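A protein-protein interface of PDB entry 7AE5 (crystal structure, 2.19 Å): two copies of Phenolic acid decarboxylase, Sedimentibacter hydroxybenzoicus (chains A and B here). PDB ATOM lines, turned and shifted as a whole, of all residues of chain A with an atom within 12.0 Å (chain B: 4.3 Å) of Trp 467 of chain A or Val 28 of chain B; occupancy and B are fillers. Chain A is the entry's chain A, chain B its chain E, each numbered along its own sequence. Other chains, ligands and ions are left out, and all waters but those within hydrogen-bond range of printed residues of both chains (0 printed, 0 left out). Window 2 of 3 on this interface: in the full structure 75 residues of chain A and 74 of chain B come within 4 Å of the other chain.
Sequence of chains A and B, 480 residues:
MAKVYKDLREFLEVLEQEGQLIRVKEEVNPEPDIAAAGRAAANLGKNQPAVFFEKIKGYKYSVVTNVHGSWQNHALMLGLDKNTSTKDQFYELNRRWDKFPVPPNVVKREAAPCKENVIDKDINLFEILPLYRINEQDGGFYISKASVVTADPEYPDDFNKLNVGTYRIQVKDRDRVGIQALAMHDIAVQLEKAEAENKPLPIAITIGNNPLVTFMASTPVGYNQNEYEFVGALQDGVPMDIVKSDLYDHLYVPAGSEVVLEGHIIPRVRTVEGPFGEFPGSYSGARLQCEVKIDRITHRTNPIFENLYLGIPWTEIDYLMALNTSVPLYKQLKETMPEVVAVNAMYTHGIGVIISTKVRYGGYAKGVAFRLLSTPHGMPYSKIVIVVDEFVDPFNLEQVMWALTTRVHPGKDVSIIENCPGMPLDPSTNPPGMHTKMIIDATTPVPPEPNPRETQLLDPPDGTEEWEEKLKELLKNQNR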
ATOM      1  N   PRO A 460      12.949   5.277  -7.440  1.00  0.00           N
ATOM      2  CA  PRO A 460      13.550   5.413  -8.764  1.00  0.00           C
ATOM      3  C   PRO A 460      15.006   5.812  -8.658  1.00  0.00           C
ATOM      4  O   PRO A 460      15.419   6.475  -7.688  1.00  0.00           O
ATOM      5  CB  PRO A 460      12.709   6.517  -9.423  1.00  0.00           C
ATOM      6  CG  PRO A 460      12.067   7.248  -8.284  1.00  0.00           C
ATOM      7  CD  PRO A 460      11.832   6.213  -7.235  1.00  0.00           C
ATOM      8  N   PRO A 461      15.829   5.423  -9.629  1.00  0.00           N
ATOM      9  CA  PRO A 461      17.246   5.789  -9.582  1.00  0.00           C
ATOM     10  C   PRO A 461      17.437   7.275  -9.828  1.00  0.00           C
ATOM     11  O   PRO A 461      16.665   7.912 -10.548  1.00  0.00           O
ATOM     12  CB  PRO A 461      17.873   4.955 -10.709  1.00  0.00           C
ATOM     13  CG  PRO A 461      16.813   3.966 -11.124  1.00  0.00           C
ATOM     14  CD  PRO A 461      15.508   4.620 -10.819  1.00  0.00           C
ATOM     15  N   ASP A 462      18.476   7.826  -9.203  1.00  0.00           N
ATOM     16  CA  ASP A 462      18.806   9.228  -9.408  1.00  0.00           C
ATOM     17  C   ASP A 462      19.007   9.497 -10.892  1.00  0.00           C
ATOM     18  O   ASP A 462      19.605   8.692 -11.611  1.00  0.00           O
ATOM     19  CB  ASP A 462      20.067   9.604  -8.630  1.00  0.00           C
ATOM     20  CG  ASP A 462      19.864   9.557  -7.131  1.00  0.00           C
ATOM     21  OD1 ASP A 462      18.717   9.757  -6.677  1.00  0.00           O
ATOM     22  OD2 ASP A 462      20.856   9.329  -6.407  1.00  0.00           O
ATOM     23  N   GLY A 463      18.487  10.622 -11.357  1.00  0.00           N
ATOM     24  CA  GLY A 463      18.554  10.929 -12.766  1.00  0.00           C
ATOM     25  C   GLY A 463      17.348  10.510 -13.570  1.00  0.00           C
ATOM     26  O   GLY A 463      17.395  10.579 -14.804  1.00  0.00           O
ATOM     27  N   THR A 464      16.258  10.102 -12.918  1.00  0.00           N
ATOM     28  CA  THR A 464      15.113   9.574 -13.653  1.00  0.00           C
ATOM     29  C   THR A 464      14.429  10.656 -14.482  1.00  0.00           C
ATOM     30  O   THR A 464      14.135  10.448 -15.665  1.00  0.00           O
ATOM     31  CB  THR A 464      14.121   8.925 -12.687  1.00  0.00           C
ATOM     32  OG1 THR A 464      14.675   7.702 -12.188  1.00  0.00           O
ATOM     33  CG2 THR A 464      12.808   8.626 -13.395  1.00  0.00           C
ATOM     34  N   GLU A 465      14.163  11.819 -13.883  1.00  0.00           N
ATOM     35  CA  GLU A 465      13.432  12.858 -14.603  1.00  0.00           C
ATOM     36  C   GLU A 465      14.260  13.423 -15.752  1.00  0.00           C
ATOM     37  O   GLU A 465      13.751  13.592 -16.866  1.00  0.00           O
ATOM     38  CB  GLU A 465      12.999  13.966 -13.641  1.00  0.00           C
ATOM     39  CG  GLU A 465      11.655  14.601 -13.993  1.00  0.00           C
ATOM     40  CD  GLU A 465      10.461  13.731 -13.614  1.00  0.00           C
ATOM     41  OE1 GLU A 465       9.312  14.189 -13.796  1.00  0.00           O
ATOM     42  OE2 GLU A 465      10.666  12.595 -13.131  1.00  0.00           O
ATOM     43  N   GLU A 466      15.543  13.716 -15.502  1.00  0.00           N
ATOM     44  CA  GLU A 466      16.418  14.209 -16.568  1.00  0.00           C
ATOM     45  C   GLU A 466      16.475  13.223 -17.727  1.00  0.00           C
ATOM     46  O   GLU A 466      16.410  13.626 -18.895  1.00  0.00           O
ATOM     47  CB  GLU A 466      17.833  14.488 -16.038  1.00  0.00           C
ATOM     48  CG  GLU A 466      17.948  15.268 -14.716  1.00  0.00           C
ATOM     49  CD  GLU A 466      17.463  14.468 -13.524  1.00  0.00           C
ATOM     50  OE1 GLU A 466      17.043  13.314 -13.745  1.00  0.00           O
ATOM     51  OE2 GLU A 466      17.528  14.969 -12.378  1.00  0.00           O
ATOM     52  N   TRP A 467      16.583  11.927 -17.426  1.00  0.00           N
ATOM     53  CA  TRP A 467      16.588  10.923 -18.486  1.00  0.00           C
ATOM     54  C   TRP A 467      15.236  10.831 -19.177  1.00  0.00           C
ATOM     55  O   TRP A 467      15.170  10.448 -20.351  1.00  0.00           O
ATOM     56  CB  TRP A 467      16.991   9.563 -17.923  1.00  0.00           C
ATOM     57  CG  TRP A 467      18.462   9.342 -17.950  1.00  0.00           C
ATOM     58  CD1 TRP A 467      19.323   9.424 -16.895  1.00  0.00           C
ATOM     59  CD2 TRP A 467      19.259   9.015 -19.095  1.00  0.00           C
ATOM     60  NE1 TRP A 467      20.605   9.161 -17.310  1.00  0.00           N
ATOM     61  CE2 TRP A 467      20.593   8.907 -18.656  1.00  0.00           C
ATOM     62  CE3 TRP A 467      18.973   8.799 -20.447  1.00  0.00           C
ATOM     63  CZ2 TRP A 467      21.641   8.594 -19.521  1.00  0.00           C
ATOM     64  CZ3 TRP A 467      20.013   8.486 -21.304  1.00  0.00           C
ATOM     65  CH2 TRP A 467      21.331   8.388 -20.837  1.00  0.00           C
ATOM     66  N   GLU A 468      14.153  11.170 -18.474  1.00  0.00           N
ATOM     67  CA  GLU A 468      12.845  11.205 -19.118  1.00  0.00           C
ATOM     68  C   GLU A 468      12.834  12.211 -20.261  1.00  0.00           C
ATOM     69  O   GLU A 468      12.519  11.861 -21.402  1.00  0.00           O
ATOM     70  CB  GLU A 468      11.756  11.528 -18.093  1.00  0.00           C
ATOM     71  CG  GLU A 468      11.138  10.298 -17.443  1.00  0.00           C
ATOM     72  CD  GLU A 468       9.967  10.636 -16.543  1.00  0.00           C
ATOM     73  OE1 GLU A 468       9.266  11.630 -16.824  1.00  0.00           O
ATOM     74  OE2 GLU A 468       9.751   9.908 -15.550  1.00  0.00           O
ATOM     75  N   GLU A 469      13.212  13.463 -19.979  1.00  0.00           N
ATOM     76  CA  GLU A 469      13.246  14.481 -21.027  1.00  0.00           C
ATOM     77  C   GLU A 469      14.213  14.104 -22.142  1.00  0.00           C
ATOM     78  O   GLU A 469      13.926  14.331 -23.323  1.00  0.00           O
ATOM     79  CB  GLU A 469      13.630  15.846 -20.451  1.00  0.00           C
ATOM     80  CG  GLU A 469      12.793  16.326 -19.280  1.00  0.00           C
ATOM     81  CD  GLU A 469      13.636  16.906 -18.159  1.00  0.00           C
ATOM     82  OE1 GLU A 469      13.690  18.147 -18.037  1.00  0.00           O
ATOM     83  OE2 GLU A 469      14.239  16.128 -17.398  1.00  0.00           O
ATOM     84  N   LYS A 470      15.371  13.536 -21.790  1.00  0.00           N
ATOM     85  CA  LYS A 470      16.369  13.209 -22.804  1.00  0.00           C
ATOM     86  C   LYS A 470      15.859  12.140 -23.763  1.00  0.00           C
ATOM     87  O   LYS A 470      16.149  12.187 -24.965  1.00  0.00           O
ATOM     88  CB  LYS A 470      17.671  12.758 -22.138  1.00  0.00           C
ATOM     89  CG  LYS A 470      18.797  12.469 -23.122  1.00  0.00           C
ATOM     90  CD  LYS A 470      20.175  12.737 -22.526  1.00  0.00           C
ATOM     91  CE  LYS A 470      20.242  12.344 -21.058  1.00  0.00           C
ATOM     92  NZ  LYS A 470      21.162  13.233 -20.290  1.00  0.00           N
ATOM     93  N   LEU A 471      15.095  11.172 -23.255  1.00  0.00           N
ATOM     94  CA  LEU A 471      14.558  10.136 -24.131  1.00  0.00           C
ATOM     95  C   LEU A 471      13.483  10.698 -25.055  1.00  0.00           C
ATOM     96  O   LEU A 471      13.445  10.356 -26.242  1.00  0.00           O
ATOM     97  CB  LEU A 471      14.012   8.974 -23.301  1.00  0.00           C
ATOM     98  CG  LEU A 471      15.070   8.118 -22.599  1.00  0.00           C
ATOM     99  CD1 LEU A 471      14.444   6.883 -21.964  1.00  0.00           C
ATOM    100  CD2 LEU A 471      16.177   7.726 -23.566  1.00  0.00           C
ATOM    101  N   LYS A 472      12.607  11.566 -24.533  1.00  0.00           N
ATOM    102  CA  LYS A 472      11.576  12.168 -25.376  1.00  0.00           C
ATOM    103  C   LYS A 472      12.190  13.001 -26.493  1.00  0.00           C
ATOM    104  O   LYS A 472      11.707  12.974 -27.631  1.00  0.00           O
ATOM    105  CB  LYS A 472      10.623  13.028 -24.542  1.00  0.00           C
ATOM    106  CG  LYS A 472      10.256  12.439 -23.199  1.00  0.00           C
ATOM    107  CD  LYS A 472       9.470  13.418 -22.342  1.00  0.00           C
ATOM    108  CE  LYS A 472       8.328  12.725 -21.622  1.00  0.00           C
ATOM    109  NZ  LYS A 472       7.261  13.673 -21.203  1.00  0.00           N
ATOM    110  N   GLU A 473      13.254  13.749 -26.191  1.00  0.00           N
ATOM    111  CA  GLU A 473      13.878  14.569 -27.224  1.00  0.00           C
ATOM    112  C   GLU A 473      14.638  13.715 -28.231  1.00  0.00           C
ATOM    113  O   GLU A 473      14.762  14.102 -29.400  1.00  0.00           O
ATOM    114  CB  GLU A 473      14.793  15.619 -26.588  1.00  0.00           C
ATOM    115  CG  GLU A 473      16.224  15.175 -26.344  1.00  0.00           C
ATOM    116  CD  GLU A 473      17.043  16.237 -25.636  1.00  0.00           C
ATOM    117  OE1 GLU A 473      16.477  17.300 -25.304  1.00  0.00           O
ATOM    118  OE2 GLU A 473      18.251  16.010 -25.414  1.00  0.00           O
ATOM    119  N   LEU A 474      15.143  12.553 -27.807  1.00  0.00           N
ATOM    120  CA  LEU A 474      15.700  11.610 -28.769  1.00  0.00           C
ATOM    121  C   LEU A 474      14.598  10.935 -29.573  1.00  0.00           C
ATOM    122  O   LEU A 474      14.814  10.568 -30.732  1.00  0.00           O
ATOM    123  CB  LEU A 474      16.558  10.564 -28.053  1.00  0.00           C
ATOM    124  N   LEU A 475      13.412  10.773 -28.978  1.00  0.00           N
ATOM    125  CA  LEU A 475      12.270  10.247 -29.718  1.00  0.00           C
ATOM    126  C   LEU A 475      11.831  11.196 -30.824  1.00  0.00           C
ATOM    127  O   LEU A 475      11.388  10.745 -31.887  1.00  0.00           O
ATOM    128  CB  LEU A 475      11.104   9.989 -28.763  1.00  0.00           C
ATOM    129  CG  LEU A 475      11.036   8.636 -28.052  1.00  0.00           C
ATOM    130  CD1 LEU A 475       9.674   8.447 -27.401  1.00  0.00           C
ATOM    131  CD2 LEU A 475      11.326   7.505 -29.028  1.00  0.00           C
ATOM    132  N   LYS A 476      11.950  12.506 -30.596  1.00  0.00           N
ATOM    133  CA  LYS A 476      11.398  13.477 -31.535  1.00  0.00           C
ATOM    134  C   LYS A 476      12.208  13.544 -32.822  1.00  0.00           C
ATOM    135  O   LYS A 476      11.638  13.682 -33.910  1.00  0.00           O
ATOM    136  CB  LYS A 476      11.320  14.854 -30.876  1.00  0.00           C
ATOM    137  N   ASN A 477      13.536  13.452 -32.730  1.00  0.00           N
ATOM    138  CA  ASN A 477      14.388  13.625 -33.899  1.00  0.00           C
ATOM    139  C   ASN A 477      14.781  12.300 -34.552  1.00  0.00           C
ATOM    140  O   ASN A 477      15.764  12.249 -35.299  1.00  0.00           O
ATOM    141  CB  ASN A 477      15.620  14.467 -33.538  1.00  0.00           C
ATOM    142  CG  ASN A 477      16.640  13.718 -32.701  1.00  0.00           C
ATOM    143  OD1 ASN A 477      17.406  12.902 -33.211  1.00  0.00           O
ATOM    144  ND2 ASN A 477      16.666  14.010 -31.407  1.00  0.00           N
ATOM    145  N   GLN A 478      14.023  11.235 -34.303  1.00  0.00           N
ATOM    146  CA  GLN A 478      14.085  10.048 -35.155  1.00  0.00           C
ATOM    147  C   GLN A 478      12.770   9.904 -35.910  1.00  0.00           C
ATOM    148  O   GLN A 478      11.704   9.824 -35.298  1.00  0.00           O
ATOM    149  CB  GLN A 478      14.363   8.769 -34.357  1.00  0.00           C
ATOM    150  CG  GLN A 478      15.390   8.858 -33.233  1.00  0.00           C
ATOM    151  CD  GLN A 478      16.667   9.591 -33.604  1.00  0.00           C
ATOM    152  OE1 GLN A 478      17.239  10.297 -32.776  1.00  0.00           O
ATOM    153  NE2 GLN A 478      17.135   9.409 -34.836  1.00  0.00           N
ATOM    154  N   VAL B  24      21.421   5.730 -27.592  1.00  0.00           N
ATOM    155  CA  VAL B  24      22.183   6.703 -26.818  1.00  0.00           C
ATOM    156  C   VAL B  24      23.614   6.641 -27.341  1.00  0.00           C
ATOM    157  O   VAL B  24      24.360   5.707 -27.041  1.00  0.00           O
ATOM    158  CB  VAL B  24      22.107   6.429 -25.315  1.00  0.00           C
ATOM    159  CG1 VAL B  24      23.001   7.399 -24.554  1.00  0.00           C
ATOM    160  CG2 VAL B  24      20.669   6.538 -24.827  1.00  0.00           C
ATOM    161  N   GLU B  26      26.195   8.884 -26.975  1.00  0.00           N
ATOM    162  CA  GLU B  26      27.270   9.410 -26.147  1.00  0.00           C
ATOM    163  C   GLU B  26      27.525   8.507 -24.945  1.00  0.00           C
ATOM    164  O   GLU B  26      26.657   7.751 -24.502  1.00  0.00           O
ATOM    165  CB  GLU B  26      26.949  10.832 -25.686  1.00  0.00           C
ATOM    166  CG  GLU B  26      25.779  10.931 -24.721  1.00  0.00           C
ATOM    167  CD  GLU B  26      24.439  11.023 -25.428  1.00  0.00           C
ATOM    168  OE1 GLU B  26      23.587  11.819 -24.980  1.00  0.00           O
ATOM    169  OE2 GLU B  26      24.234  10.296 -26.423  1.00  0.00           O
ATOM    170  N   GLU B  27      28.743   8.603 -24.419  1.00  0.00           N
ATOM    171  CA  GLU B  27      29.171   7.744 -23.325  1.00  0.00           C
ATOM    172  C   GLU B  27      28.360   8.022 -22.064  1.00  0.00           C
ATOM    173  O   GLU B  27      28.105   9.176 -21.709  1.00  0.00           O
ATOM    174  CB  GLU B  27      30.661   7.958 -23.057  1.00  0.00           C
ATOM    175  CG  GLU B  27      31.249   7.110 -21.946  1.00  0.00           C
ATOM    176  CD  GLU B  27      32.677   7.508 -21.626  1.00  0.00           C
ATOM    177  OE1 GLU B  27      32.865   8.496 -20.884  1.00  0.00           O
ATOM    178  OE2 GLU B  27      33.609   6.840 -22.123  1.00  0.00           O
ATOM    179  N   VAL B  28      27.955   6.952 -21.387  1.00  0.00           N
ATOM    180  CA  VAL B  28      27.186   7.046 -20.154  1.00  0.00           C
ATOM    181  C   VAL B  28      27.998   6.439 -19.021  1.00  0.00           C
ATOM    182  O   VAL B  28      28.861   5.582 -19.236  1.00  0.00           O
ATOM    183  CB  VAL B  28      25.814   6.344 -20.263  1.00  0.00           C
ATOM    184  CG1 VAL B  28      24.900   7.099 -21.214  1.00  0.00           C
ATOM    185  CG2 VAL B  28      25.987   4.896 -20.702  1.00  0.00           C
ATOM    186  N   ASN B  29      27.718   6.898 -17.808  1.00  0.00           N
ATOM    187  CA  ASN B  29      28.242   6.220 -16.637  1.00  0.00           C
ATOM    188  C   ASN B  29      27.418   4.964 -16.365  1.00  0.00           C
ATOM    189  O   ASN B  29      26.214   4.938 -16.633  1.00  0.00           O
ATOM    190  CB  ASN B  29      28.202   7.138 -15.420  1.00  0.00           C
ATOM    191  CG  ASN B  29      29.440   7.998 -15.298  1.00  0.00           C
ATOM    192  OD1 ASN B  29      29.567   9.021 -15.969  1.00  0.00           O
ATOM    193  ND2 ASN B  29      30.365   7.587 -14.437  1.00  0.00           N
ATOM    194  N   PRO B  30      28.047   3.903 -15.856  1.00  0.00           N
ATOM    195  CA  PRO B  30      27.269   2.701 -15.505  1.00  0.00           C
ATOM    196  C   PRO B  30      26.136   2.993 -14.533  1.00  0.00           C
ATOM    197  O   PRO B  30      25.003   2.543 -14.744  1.00  0.00           O
ATOM    198  CB  PRO B  30      28.328   1.761 -14.906  1.00  0.00           C
ATOM    199  CG  PRO B  30      29.532   2.626 -14.635  1.00  0.00           C
ATOM    200  CD  PRO B  30      29.491   3.713 -15.651  1.00  0.00           C
ATOM    201  N   ASP B  33      23.053   5.994 -14.696  1.00  0.00           N
ATOM    202  CA  ASP B  33      22.514   6.343 -16.009  1.00  0.00           C
ATOM    203  C   ASP B  33      21.676   5.211 -16.595  1.00  0.00           C
ATOM    204  O   ASP B  33      20.533   5.425 -17.017  1.00  0.00           O
ATOM    205  CB  ASP B  33      23.653   6.707 -16.962  1.00  0.00           C
ATOM    206  CG  ASP B  33      24.295   8.041 -16.630  1.00  0.00           C
ATOM    207  OD1 ASP B  33      23.794   8.739 -15.723  1.00  0.00           O
ATOM    208  OD2 ASP B  33      25.306   8.392 -17.277  1.00  0.00           O
ATOM    209  N   ALA B  36      18.505   4.617 -14.548  1.00  0.00           N
ATOM    210  CA  ALA B  36      17.596   5.751 -14.678  1.00  0.00           C
ATOM    211  C   ALA B  36      16.970   5.800 -16.065  1.00  0.00           C
ATOM    212  O   ALA B  36      15.801   6.178 -16.213  1.00  0.00           O
ATOM    213  CB  ALA B  36      18.328   7.057 -14.375  1.00  0.00           C
ATOM    214  N   ALA B  37      17.729   5.421 -17.096  1.00  0.00           N
ATOM    215  CA  ALA B  37      17.169   5.384 -18.442  1.00  0.00           C
ATOM    216  C   ALA B  37      16.109   4.297 -18.566  1.00  0.00           C
ATOM    217  O   ALA B  37      15.054   4.518 -19.173  1.00  0.00           O
ATOM    218  CB  ALA B  37      18.279   5.175 -19.470  1.00  0.00           C
ATOM    219  N   ALA B  40      13.196   5.619 -16.798  1.00  0.00           N
ATOM    220  CA  ALA B  40      12.604   6.696 -17.585  1.00  0.00           C
ATOM    221  C   ALA B  40      11.862   6.154 -18.801  1.00  0.00           C
ATOM    222  O   ALA B  40      10.782   6.649 -19.145  1.00  0.00           O
ATOM    223  CB  ALA B  40      13.682   7.689 -18.015  1.00  0.00           C
ATOM    224  N   PHE B  53      22.582   1.556 -25.386  1.00  0.00           N
ATOM    225  CA  PHE B  53      23.720   2.393 -25.018  1.00  0.00           C
ATOM    226  C   PHE B  53      24.934   1.969 -25.836  1.00  0.00           C
ATOM    227  O   PHE B  53      25.469   0.873 -25.642  1.00  0.00           O
ATOM    228  CB  PHE B  53      24.015   2.287 -23.525  1.00  0.00           C
ATOM    229  CG  PHE B  53      22.871   2.697 -22.654  1.00  0.00           C
ATOM    230  CD1 PHE B  53      22.612   4.035 -22.415  1.00  0.00           C
ATOM    231  CD2 PHE B  53      22.053   1.743 -22.076  1.00  0.00           C
ATOM    232  CE1 PHE B  53      21.556   4.414 -21.613  1.00  0.00           C
ATOM    233  CE2 PHE B  53      20.997   2.116 -21.274  1.00  0.00           C
ATOM    234  CZ  PHE B  53      20.749   3.452 -21.043  1.00  0.00           C
ATOM    235  N   LYS B  55      27.953   3.341 -25.798  1.00  0.00           N
ATOM    236  CA  LYS B  55      29.207   3.467 -25.067  1.00  0.00           C
ATOM    237  C   LYS B  55      28.927   3.681 -23.589  1.00  0.00           C
ATOM    238  O   LYS B  55      28.104   4.526 -23.224  1.00  0.00           O
ATOM    239  CB  LYS B  55      30.051   4.624 -25.616  1.00  0.00           C
ATOM    240  N   ILE B  56      29.615   2.913 -22.746  1.00  0.00           N
ATOM    241  CA  ILE B  56      29.554   3.053 -21.297  1.00  0.00           C
ATOM    242  C   ILE B  56      30.970   3.260 -20.779  1.00  0.00           C
ATOM    243  O   ILE B  56      31.924   2.681 -21.311  1.00  0.00           O
ATOM    244  CB  ILE B  56      28.893   1.828 -20.628  1.00  0.00           C
ATOM    245  CG1 ILE B  56      27.569   1.491 -21.315  1.00  0.00           C
ATOM    246  CG2 ILE B  56      28.656   2.083 -19.149  1.00  0.00           C
ATOM    247  CD1 ILE B  56      27.567   0.156 -22.018  1.00  0.00           C
ATOM    248  N   LYS B  57      31.101   4.090 -19.745  1.00  0.00           N
ATOM    249  CA  LYS B  57      32.409   4.449 -19.209  1.00  0.00           C
ATOM    250  C   LYS B  57      33.167   3.217 -18.732  1.00  0.00           C
ATOM    251  O   LYS B  57      32.671   2.454 -17.897  1.00  0.00           O
ATOM    252  CB  LYS B  57      32.240   5.443 -18.059  1.00  0.00           C
ATOM    253  CG  LYS B  57      32.998   6.749 -18.234  1.00  0.00           C
ATOM    254  CD  LYS B  57      32.693   7.713 -17.100  1.00  0.00           C
ATOM    255  CE  LYS B  57      32.314   9.089 -17.625  1.00  0.00           C
ATOM    256  NZ  LYS B  57      31.914  10.012 -16.525  1.00  0.00           N
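Of chain B, only Val 28 (3.8 Å), Asp 33 (3.6 Å), Ala 36 (3.6 Å), Ala 37 (3.8 Å) and Ala 40 (3.7 Å) come within 4 Å of Trp 467 of chain A. Printed residues of chain A within 4 Å of Val 28 of chain B: Trp 467 (3.8 Å). No residue of chain A comes within 4 Å of Glu 26 of chain B. No residue of chain A comes within 4 Å of Asn 29 of chain B. No residue of chain A comes within 4 Å of Pro 30 of chain B. Asp 33 of chain B touches one residue of chain A. Of chain A, only Trp 467 (3.8 Å) and Leu 471 (3.7 Å) come within 4 Å of Ala 37 of chain B. No residue of chain A comes within 4 Å of Phe 53 of chain B. Lys 55 of chain B touches none of the printed residues of chain A. No residue of chain A comes within 4 Å of Ile 56 of chain B. No residue of chain A comes within 4 Å of Lys 57 of chain B. Printed residues of chain B within 4 Å of Thr 464 of chain A: Ala 36 (3.96 Å) and Ala 40 (3.7 Å). Of the printed residues of chain B, Asp 462 of chain A touches Ala 36. Lys 470 of chain A touches none of the printed residues of chain B. The nearest printed residue of chain B that does not touch Trp 467 of chain A is Phe 53 of chain B (4.1 Å).
No position is printed for both chains. Of the 12 pairs that touch across the chains among the printed residues, none has its exchanged pair printed and touching as well.
The backbone NH (N) of Val 28 of chain B lies within hydrogen-bond range of the backbone carbonyl oxygen (O) of Lys 55 of chain B, 3.0 Å away. The backbone carbonyl oxygen (O) of Val 28 of chain B is in hydrogen-bond range of the backbone NH (N) of Lys 57 of chain B, at 2.7 Å. The backbone NH (N) of Asn 29 of chain B is in hydrogen-bond range of the side-chain carboxylate (OD2) of Asp 33 of chain B (2.9 Å). The backbone carbonyl oxygen of Pro 461 of chain A is in hydrogen-bond range of the side-chain hydroxyl of Thr 464 of chain A. The side-chain carboxylate (OE1) of Glu 466 of chain A lies within hydrogen-bond range of the backbone NH (N) of Thr 464 of chain A (3.4 Å).
Ala 36 of chain B touches Pro 461 of chain A. Ala 36 of chain B touches Asp 462 of chain A. Gly 463 of chain A touches Ala 36 of chain B. N of Thr 464 of chain A touches CB of Ala 36 of chain B, at 3.96 Å. O of Thr 464 of chain A touches CB of Ala 40 of chain B (3.7 Å). CH2 of Trp 467 of chain A touches CG1 of Val 28 of chain B, 3.8 Å away. Trp 467 of chain A touches Asp 33 of chain B. CD1 of Trp 467 of chain A touches CB of Ala 36 of chain B, at 3.6 Å. Trp 467 of chain A touches Ala 40 of chain B (C to CB, 3.7 Å). CD1 of Leu 471 of chain A touches O of Ala 37 of chain B (3.7 Å).
Of the 14 printed residues of chain B, 5 touch a printed residue of chain A. Printed residues of chain B that touch a printed residue of chain A: Val 28, Asp 33, Ala 36, Ala 37 and Ala 40. Hydrophobic or aromatic side chains of chain B that line the printed part of chain A: Val 28, Ala 36, Ala 37 and Ala 40. Along chain B the printed residues that touch a printed residue of chain A span positions 28 to 40. Of the 19 printed residues of chain A, 7 touch a printed residue of chain B. Hydrophobic or aromatic side chains of chain A within 4 Å of the printed part of chain B: Pro 461, Trp 467 and Leu 471. Among the printed residues, no Asp or Glu carboxylate lies within 4 Å of a Lys or Arg side-chain nitrogen of the other chain.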
